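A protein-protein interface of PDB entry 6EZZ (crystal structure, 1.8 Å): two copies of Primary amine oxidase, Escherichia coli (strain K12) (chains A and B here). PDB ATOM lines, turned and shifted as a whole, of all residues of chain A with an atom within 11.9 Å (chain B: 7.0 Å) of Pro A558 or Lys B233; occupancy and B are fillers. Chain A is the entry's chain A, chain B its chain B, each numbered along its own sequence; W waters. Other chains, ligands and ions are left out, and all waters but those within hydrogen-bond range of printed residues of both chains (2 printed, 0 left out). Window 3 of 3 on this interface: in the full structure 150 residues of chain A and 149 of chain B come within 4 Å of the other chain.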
ATOM      1  N   LYS A 551      11.082  31.881 -15.076  1.00  0.00           N
ATOM      2  CA  LYS A 551      10.953  33.255 -15.580  1.00  0.00           C
ATOM      3  C   LYS A 551      11.021  33.297 -17.117  1.00  0.00           C
ATOM      4  O   LYS A 551      11.661  32.447 -17.752  1.00  0.00           O
ATOM      5  CB  LYS A 551      12.086  34.141 -15.030  1.00  0.00           C
ATOM      6  CG  LYS A 551      12.014  34.407 -13.537  1.00  0.00           C
ATOM      7  CD  LYS A 551      12.911  35.572 -13.169  1.00  0.00           C
ATOM      8  CE  LYS A 551      13.043  35.728 -11.665  1.00  0.00           C
ATOM      9  NZ  LYS A 551      11.794  36.268 -11.070  1.00  0.00           N
ATOM     10  N   PRO A 552      10.404  34.322 -17.738  1.00  0.00           N
ATOM     11  CA  PRO A 552      10.553  34.459 -19.199  1.00  0.00           C
ATOM     12  C   PRO A 552      12.013  34.595 -19.645  1.00  0.00           C
ATOM     13  O   PRO A 552      12.851  35.195 -18.944  1.00  0.00           O
ATOM     14  CB  PRO A 552       9.775  35.762 -19.515  1.00  0.00           C
ATOM     15  CG  PRO A 552       8.830  35.939 -18.348  1.00  0.00           C
ATOM     16  CD  PRO A 552       9.596  35.420 -17.157  1.00  0.00           C
ATOM     17  N   ASN A 553      12.335  34.001 -20.796  1.00  0.00           N
ATOM     18  CA  ASN A 553      13.644  34.153 -21.388  1.00  0.00           C
ATOM     19  C   ASN A 553      13.792  35.550 -22.024  1.00  0.00           C
ATOM     20  O   ASN A 553      13.007  35.923 -22.886  1.00  0.00           O
ATOM     21  CB  ASN A 553      13.834  33.097 -22.462  1.00  0.00           C
ATOM     22  CG  ASN A 553      15.150  33.207 -23.167  1.00  0.00           C
ATOM     23  OD1 ASN A 553      16.133  33.741 -22.632  1.00  0.00           O
ATOM     24  ND2 ASN A 553      15.191  32.678 -24.401  1.00  0.00           N
ATOM     25  N   THR A 554      14.829  36.267 -21.628  1.00  0.00           N
ATOM     26  CA  THR A 554      15.180  37.576 -22.194  1.00  0.00           C
ATOM     27  C   THR A 554      16.540  37.534 -22.887  1.00  0.00           C
ATOM     28  O   THR A 554      17.065  38.576 -23.267  1.00  0.00           O
ATOM     29  CB  THR A 554      15.249  38.651 -21.075  1.00  0.00           C
ATOM     30  OG1 THR A 554      16.255  38.291 -20.117  1.00  0.00           O
ATOM     31  CG2 THR A 554      13.898  38.765 -20.352  1.00  0.00           C
ATOM     32  N   ALA A 555      17.135  36.343 -23.034  1.00  0.00           N
ATOM     33  CA  ALA A 555      18.479  36.225 -23.619  1.00  0.00           C
ATOM     34  C   ALA A 555      18.446  35.885 -25.113  1.00  0.00           C
ATOM     35  O   ALA A 555      19.496  35.826 -25.741  1.00  0.00           O
ATOM     36  CB  ALA A 555      19.293  35.183 -22.861  1.00  0.00           C
ATOM     37  N   GLY A 556      17.264  35.634 -25.667  1.00  0.00           N
ATOM     38  CA  GLY A 556      17.120  35.277 -27.074  1.00  0.00           C
ATOM     39  C   GLY A 556      17.116  33.778 -27.328  1.00  0.00           C
ATOM     40  O   GLY A 556      17.248  32.962 -26.401  1.00  0.00           O
ATOM     41  N   GLY A 557      16.963  33.415 -28.592  1.00  0.00           N
ATOM     42  CA  GLY A 557      16.950  32.019 -28.995  1.00  0.00           C
ATOM     43  C   GLY A 557      15.587  31.425 -28.744  1.00  0.00           C
ATOM     44  O   GLY A 557      14.668  32.122 -28.290  1.00  0.00           O
ATOM     45  N   PRO A 558      15.428  30.117 -29.023  1.00  0.00           N
ATOM     46  CA  PRO A 558      14.086  29.561 -29.062  1.00  0.00           C
ATOM     47  C   PRO A 558      13.334  29.358 -27.735  1.00  0.00           C
ATOM     48  O   PRO A 558      12.089  29.196 -27.755  1.00  0.00           O
ATOM     49  CB  PRO A 558      14.287  28.207 -29.785  1.00  0.00           C
ATOM     50  CG  PRO A 558      15.566  28.358 -30.528  1.00  0.00           C
ATOM     51  CD  PRO A 558      16.412  29.238 -29.685  1.00  0.00           C
ATOM     52  N   ARG A 559      14.039  29.361 -26.606  1.00  0.00           N
ATOM     53  CA  ARG A 559      13.342  29.094 -25.317  1.00  0.00           C
ATOM     54  C   ARG A 559      12.429  30.272 -24.930  1.00  0.00           C
ATOM     55  O   ARG A 559      12.811  31.436 -25.076  1.00  0.00           O
ATOM     56  CB  ARG A 559      14.337  28.824 -24.183  1.00  0.00           C
ATOM     57  CG  ARG A 559      14.935  27.423 -24.246  1.00  0.00           C
ATOM     58  CD  ARG A 559      13.986  26.385 -23.684  1.00  0.00           C
ATOM     59  NE  ARG A 559      14.013  26.431 -22.215  1.00  0.00           N
ATOM     60  CZ  ARG A 559      14.937  25.848 -21.433  1.00  0.00           C
ATOM     61  NH1 ARG A 559      15.938  25.124 -21.939  1.00  0.00           N
ATOM     62  NH2 ARG A 559      14.843  25.976 -20.117  1.00  0.00           N
ATOM     63  N   THR A 560      11.234  29.944 -24.476  1.00  0.00           N
ATOM     64  CA  THR A 560      10.309  30.950 -23.927  1.00  0.00           C
ATOM     65  C   THR A 560      10.556  31.158 -22.437  1.00  0.00           C
ATOM     66  O   THR A 560      10.194  32.224 -21.899  1.00  0.00           O
ATOM     67  CB  THR A 560       8.851  30.557 -24.125  1.00  0.00           C
ATOM     68  OG1 THR A 560       8.504  29.487 -23.237  1.00  0.00           O
ATOM     69  CG2 THR A 560       8.576  30.169 -25.559  1.00  0.00           C
ATOM     70  N   SER A 561      11.183  30.176 -21.758  1.00  0.00           N
ATOM     71  CA  SER A 561      11.357  30.254 -20.283  1.00  0.00           C
ATOM     72  C   SER A 561      12.703  29.718 -19.783  1.00  0.00           C
ATOM     73  O   SER A 561      13.465  29.081 -20.529  1.00  0.00           O
ATOM     74  CB  SER A 561      10.202  29.558 -19.578  1.00  0.00           C
ATOM     75  OG  SER A 561      10.350  28.138 -19.616  1.00  0.00           O
ATOM     76  N   THR A 562      13.025  30.093 -18.551  1.00  0.00           N
ATOM     77  CA  THR A 562      14.306  29.776 -17.937  1.00  0.00           C
ATOM     78  C   THR A 562      14.117  29.408 -16.451  1.00  0.00           C
ATOM     79  O   THR A 562      13.096  29.776 -15.832  1.00  0.00           O
ATOM     80  CB  THR A 562      15.313  30.938 -18.043  1.00  0.00           C
ATOM     81  OG1 THR A 562      14.913  32.049 -17.200  1.00  0.00           O
ATOM     82  CG2 THR A 562      15.487  31.394 -19.501  1.00  0.00           C
ATOM     83  N   TYR B 229      12.938  19.303 -30.534  1.00  0.00           N
ATOM     84  CA  TYR B 229      12.082  19.864 -31.582  1.00  0.00           C
ATOM     85  C   TYR B 229      11.639  21.266 -31.185  1.00  0.00           C
ATOM     86  O   TYR B 229      11.169  21.458 -30.058  1.00  0.00           O
ATOM     87  CB  TYR B 229      10.877  18.976 -31.778  1.00  0.00           C
ATOM     88  CG  TYR B 229       9.923  19.505 -32.804  1.00  0.00           C
ATOM     89  CD1 TYR B 229      10.239  19.436 -34.152  1.00  0.00           C
ATOM     90  CD2 TYR B 229       8.708  20.070 -32.433  1.00  0.00           C
ATOM     91  CE1 TYR B 229       9.365  19.911 -35.122  1.00  0.00           C
ATOM     92  CE2 TYR B 229       7.819  20.552 -33.388  1.00  0.00           C
ATOM     93  CZ  TYR B 229       8.152  20.473 -34.739  1.00  0.00           C
ATOM     94  OH  TYR B 229       7.287  20.944 -35.706  1.00  0.00           O
ATOM     95  N   PHE B 230      11.786  22.226 -32.111  1.00  0.00           N
ATOM     96  CA  PHE B 230      11.435  23.637 -31.883  1.00  0.00           C
ATOM     97  C   PHE B 230      10.631  24.259 -33.063  1.00  0.00           C
ATOM     98  O   PHE B 230      10.644  25.474 -33.243  1.00  0.00           O
ATOM     99  CB  PHE B 230      12.712  24.440 -31.610  1.00  0.00           C
ATOM    100  CG  PHE B 230      13.373  24.073 -30.313  1.00  0.00           C
ATOM    101  CD1 PHE B 230      12.933  24.643 -29.119  1.00  0.00           C
ATOM    102  CD2 PHE B 230      14.392  23.126 -30.270  1.00  0.00           C
ATOM    103  CE1 PHE B 230      13.503  24.297 -27.911  1.00  0.00           C
ATOM    104  CE2 PHE B 230      14.966  22.777 -29.059  1.00  0.00           C
ATOM    105  CZ  PHE B 230      14.528  23.371 -27.876  1.00  0.00           C
ATOM    106  N   ASP B 231       9.930  23.420 -33.839  1.00  0.00           N
ATOM    107  CA  ASP B 231       9.154  23.860 -35.008  1.00  0.00           C
ATOM    108  C   ASP B 231       9.946  24.860 -35.887  1.00  0.00           C
ATOM    109  O   ASP B 231       9.426  25.903 -36.285  1.00  0.00           O
ATOM    110  CB  ASP B 231       7.831  24.472 -34.514  1.00  0.00           C
ATOM    111  CG  ASP B 231       6.781  24.616 -35.611  1.00  0.00           C
ATOM    112  OD1 ASP B 231       6.960  24.080 -36.718  1.00  0.00           O
ATOM    113  OD2 ASP B 231       5.756  25.269 -35.347  1.00  0.00           O
ATOM    114  N   GLY B 232      11.221  24.554 -36.127  1.00  0.00           N
ATOM    115  CA  GLY B 232      12.066  25.322 -37.026  1.00  0.00           C
ATOM    116  C   GLY B 232      12.846  26.466 -36.426  1.00  0.00           C
ATOM    117  O   GLY B 232      13.770  26.958 -37.085  1.00  0.00           O
ATOM    118  N   LYS B 233      12.568  26.876 -35.174  1.00  0.00           N
ATOM    119  CA  LYS B 233      13.350  27.976 -34.564  1.00  0.00           C
ATOM    120  C   LYS B 233      14.791  27.664 -34.334  1.00  0.00           C
ATOM    121  O   LYS B 233      15.609  28.594 -34.249  1.00  0.00           O
ATOM    122  CB  LYS B 233      12.750  28.444 -33.233  1.00  0.00           C
ATOM    123  CG  LYS B 233      11.363  29.048 -33.371  1.00  0.00           C
ATOM    124  CD  LYS B 233      10.965  29.754 -32.099  1.00  0.00           C
ATOM    125  CE  LYS B 233       9.671  30.500 -32.302  1.00  0.00           C
ATOM    126  NZ  LYS B 233       9.273  31.058 -31.003  1.00  0.00           N
ATOM    127  N   ASP B 234      15.105  26.359 -34.190  1.00  0.00           N
ATOM    128  CA  ASP B 234      16.499  25.885 -34.147  1.00  0.00           C
ATOM    129  C   ASP B 234      17.158  25.835 -35.539  1.00  0.00           C
ATOM    130  O   ASP B 234      18.406  25.703 -35.641  1.00  0.00           O
ATOM    131  CB  ASP B 234      16.643  24.512 -33.401  1.00  0.00           C
ATOM    132  CG  ASP B 234      15.772  23.375 -33.978  1.00  0.00           C
ATOM    133  OD1 ASP B 234      14.978  23.605 -34.924  1.00  0.00           O
ATOM    134  OD2 ASP B 234      15.881  22.203 -33.469  1.00  0.00           O
ATOM    135  N   GLY B 235      16.343  25.976 -36.589  1.00  0.00           N
ATOM    136  CA  GLY B 235      16.814  26.016 -37.995  1.00  0.00           C
ATOM    137  C   GLY B 235      17.265  24.647 -38.493  1.00  0.00           C
ATOM    138  O   GLY B 235      18.230  24.538 -39.256  1.00  0.00           O
ATOM    139  N   LEU B 236      16.566  23.601 -38.045  1.00  0.00           N
ATOM    140  CA  LEU B 236      17.006  22.220 -38.242  1.00  0.00           C
ATOM    141  C   LEU B 236      15.892  21.466 -38.926  1.00  0.00           C
ATOM    142  O   LEU B 236      14.747  21.434 -38.466  1.00  0.00           O
ATOM    143  CB  LEU B 236      17.380  21.523 -36.910  1.00  0.00           C
ATOM    144  CG  LEU B 236      18.530  22.093 -36.073  1.00  0.00           C
ATOM    145  CD1 LEU B 236      18.891  21.115 -34.954  1.00  0.00           C
ATOM    146  CD2 LEU B 236      19.758  22.409 -36.918  1.00  0.00           C
ATOM    147  N   LYS B 277      26.305  22.479 -39.573  1.00  0.00           N
ATOM    148  CA  LYS B 277      26.139  23.809 -38.976  1.00  0.00           C
ATOM    149  C   LYS B 277      27.045  23.920 -37.756  1.00  0.00           C
ATOM    150  O   LYS B 277      27.138  22.972 -36.964  1.00  0.00           O
ATOM    151  CB  LYS B 277      24.666  24.043 -38.586  1.00  0.00           C
ATOM    152  CG  LYS B 277      24.395  25.462 -38.096  1.00  0.00           C
ATOM    153  CD  LYS B 277      22.948  25.654 -37.676  1.00  0.00           C
ATOM    154  CE  LYS B 277      22.637  27.138 -37.516  1.00  0.00           C
ATOM    155  NZ  LYS B 277      21.359  27.357 -36.782  1.00  0.00           N
ATOM    156  N   GLU B 279      27.354  26.579 -34.604  1.00  0.00           N
ATOM    157  CA  GLU B 279      26.805  27.732 -33.891  1.00  0.00           C
ATOM    158  C   GLU B 279      27.875  28.222 -32.924  1.00  0.00           C
ATOM    159  O   GLU B 279      28.406  27.444 -32.123  1.00  0.00           O
ATOM    160  CB  GLU B 279      25.532  27.369 -33.125  1.00  0.00           C
ATOM    161  CG  GLU B 279      24.443  26.717 -33.975  1.00  0.00           C
ATOM    162  CD  GLU B 279      23.035  26.738 -33.358  1.00  0.00           C
ATOM    163  OE1 GLU B 279      22.830  27.082 -32.151  1.00  0.00           O
ATOM    164  OE2 GLU B 279      22.099  26.402 -34.113  1.00  0.00           O
ATOM    165  N   PRO B 372      19.092  29.410 -21.321  1.00  0.00           N
ATOM    166  CA  PRO B 372      18.653  29.628 -22.713  1.00  0.00           C
ATOM    167  C   PRO B 372      19.802  29.787 -23.734  1.00  0.00           C
ATOM    168  O   PRO B 372      19.534  29.967 -24.950  1.00  0.00           O
ATOM    169  CB  PRO B 372      17.828  30.934 -22.586  1.00  0.00           C
ATOM    170  CG  PRO B 372      18.636  31.727 -21.615  1.00  0.00           C
ATOM    171  CD  PRO B 372      19.206  30.702 -20.612  1.00  0.00           C
ATOM    172  N   TYR B 377      20.032  25.530 -24.571  1.00  0.00           N
ATOM    173  CA  TYR B 377      18.579  25.688 -24.696  1.00  0.00           C
ATOM    174  C   TYR B 377      17.794  24.429 -25.077  1.00  0.00           C
ATOM    175  O   TYR B 377      16.627  24.261 -24.703  1.00  0.00           O
ATOM    176  CB  TYR B 377      18.274  26.853 -25.667  1.00  0.00           C
ATOM    177  CG  TYR B 377      18.443  26.575 -27.149  1.00  0.00           C
ATOM    178  CD1 TYR B 377      17.440  25.907 -27.867  1.00  0.00           C
ATOM    179  CD2 TYR B 377      19.561  27.024 -27.842  1.00  0.00           C
ATOM    180  CE1 TYR B 377      17.568  25.685 -29.233  1.00  0.00           C
ATOM    181  CE2 TYR B 377      19.698  26.807 -29.217  1.00  0.00           C
ATOM    182  CZ  TYR B 377      18.695  26.150 -29.899  1.00  0.00           C
ATOM    183  OH  TYR B 377      18.789  25.921 -31.251  1.00  0.00           O
ATOM    184  N   ASP B 624       4.091  26.883 -22.785  1.00  0.00           N
ATOM    185  CA  ASP B 624       4.286  27.044 -24.225  1.00  0.00           C
ATOM    186  C   ASP B 624       5.686  26.552 -24.716  1.00  0.00           C
ATOM    187  O   ASP B 624       6.012  26.710 -25.904  1.00  0.00           O
ATOM    188  CB  ASP B 624       4.016  28.511 -24.638  1.00  0.00           C
ATOM    189  CG  ASP B 624       5.032  29.492 -24.068  1.00  0.00           C
ATOM    190  OD1 ASP B 624       5.822  29.132 -23.149  1.00  0.00           O
ATOM    191  OD2 ASP B 624       5.041  30.644 -24.550  1.00  0.00           O
ATOM    192  N   GLU B 625       6.511  25.979 -23.821  1.00  0.00           N
ATOM    193  CA  GLU B 625       7.762  25.312 -24.258  1.00  0.00           C
ATOM    194  C   GLU B 625       7.453  23.982 -25.011  1.00  0.00           C
ATOM    195  O   GLU B 625       6.574  23.203 -24.615  1.00  0.00           O
ATOM    196  CB  GLU B 625       8.702  25.021 -23.070  1.00  0.00           C
ATOM    197  CG  GLU B 625       9.190  26.250 -22.288  1.00  0.00           C
ATOM    198  CD  GLU B 625      10.397  26.949 -22.890  1.00  0.00           C
ATOM    199  OE1 GLU B 625      10.519  27.024 -24.149  1.00  0.00           O
ATOM    200  OE2 GLU B 625      11.234  27.453 -22.100  1.00  0.00           O
ATOM    201  N   TRP B 626       8.207  23.712 -26.069  1.00  0.00           N
ATOM    202  CA  TRP B 626       8.045  22.463 -26.831  1.00  0.00           C
ATOM    203  C   TRP B 626       8.357  21.244 -25.962  1.00  0.00           C
ATOM    204  O   TRP B 626       7.636  20.236 -26.015  1.00  0.00           O
ATOM    205  CB  TRP B 626       8.933  22.487 -28.087  1.00  0.00           C
ATOM    206  CG  TRP B 626       8.246  23.265 -29.165  1.00  0.00           C
ATOM    207  CD1 TRP B 626       8.523  24.544 -29.593  1.00  0.00           C
ATOM    208  CD2 TRP B 626       7.128  22.828 -29.903  1.00  0.00           C
ATOM    209  NE1 TRP B 626       7.628  24.915 -30.566  1.00  0.00           N
ATOM    210  CE2 TRP B 626       6.763  23.878 -30.779  1.00  0.00           C
ATOM    211  CE3 TRP B 626       6.397  21.642 -29.927  1.00  0.00           C
ATOM    212  CZ2 TRP B 626       5.703  23.771 -31.663  1.00  0.00           C
ATOM    213  CZ3 TRP B 626       5.332  21.541 -30.807  1.00  0.00           C
ATOM    214  CH2 TRP B 626       4.996  22.603 -31.660  1.00  0.00           C
HETATM  215  O   HOH W   1      16.855  30.182 -26.127  1.00  0.00           O
HETATM  216  O   HOH W   2      10.553  31.284 -28.657  1.00  0.00           O
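Water W2 lies within hydrogen-bond range of NZ of Lys B233 (2.7 Å) and O of Pro A558 (2.7 Å).
Water W1 lies within hydrogen-bond range of O of Gly A556, O of Pro B372, N of Arg A559 and ND2 of Asn A553.
N of Thr A560 lies within hydrogen-bond range of OE1 of Glu B625, at 3.0 Å.
OG of Ser A561 is in hydrogen-bond range of OE2 of Glu B625, 2.7 Å away.
The side-chain carboxylate (OD1) of Asp B624 lies within hydrogen-bond range of the side-chain hydroxyl (OG1) of Thr A560 (2.7 Å).
O of Tyr B377 is in hydrogen-bond range of NH1 of Arg A559 (3.0 Å).
OE2 of Glu B625 lies within salt-bridge range of NE of Arg A559, at 3.0 Å.
Pro A558 touches three residues of chain B.
Of chain A, only Pro A558 (3.7 Å) comes within 4 Å of Lys B233.
Phe B230 touches just one residue of chain A: Pro A558.
No residue of chain A comes within 4 Å of Asp B234.
Of the printed residues of chain B, Thr A562 touches Pro B372 (3.8 Å).
Of the printed residues of chain B, Ala A555 touches Pro B372.
Printed residues of chain A within 4 Å of Glu B625: Arg A559 (3.0 Å), Thr A560 (3.0 Å) and Ser A561 (2.7 Å).
Glu B279 touches none of the printed residues of chain A.
Thr A554 touches none of the printed residues of chain B.
The nearest residue of chain A that does not touch Lys B233 is Thr A560 (5.6 Å).
Of the 15 printed residues of chain B, 6 touch a printed residue of chain A.
Hydrophobic or aromatic side chains of chain A that line the printed part of chain B: Ala A555 and Pro A558.
Among the printed residues, 11 pairs touch across the chains.
No position is printed for both chains.
Of the 11 pairs that touch across the chains among the printed residues, none has its exchanged pair printed and touching as well.
The side-chain amide nitrogen of Asn A553 sits at hydrogen-bond distance from the backbone carbonyl oxygen of Arg A559.
NE of Arg A559 is in hydrogen-bond range of O of Ser A561, 3.2 Å away.
The backbone carbonyl oxygen of Thr A560 lies within hydrogen-bond range of the backbone NH of Asn A553, at 3.0 Å.
ND2 of Asn A553 is in hydrogen-bond range of O of Gly A556 (2.9 Å).
The side-chain amide oxygen (OD1) of Asn A553 sits at hydrogen-bond distance from the backbone NH (N) of Ala A555 (2.8 Å).
The backbone NH (N) of Thr A562 lies within hydrogen-bond range of the backbone carbonyl oxygen (O) of Lys A551 (2.8 Å).
Among the printed residues, merely in contact across the chains: Asn A553 with Pro B372, Pro A558 with Tyr B377, Pro A558 with Lys B233, Ala A555 with Pro B372, Thr A562 with Pro B372 and Pro A558 with Phe B230.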
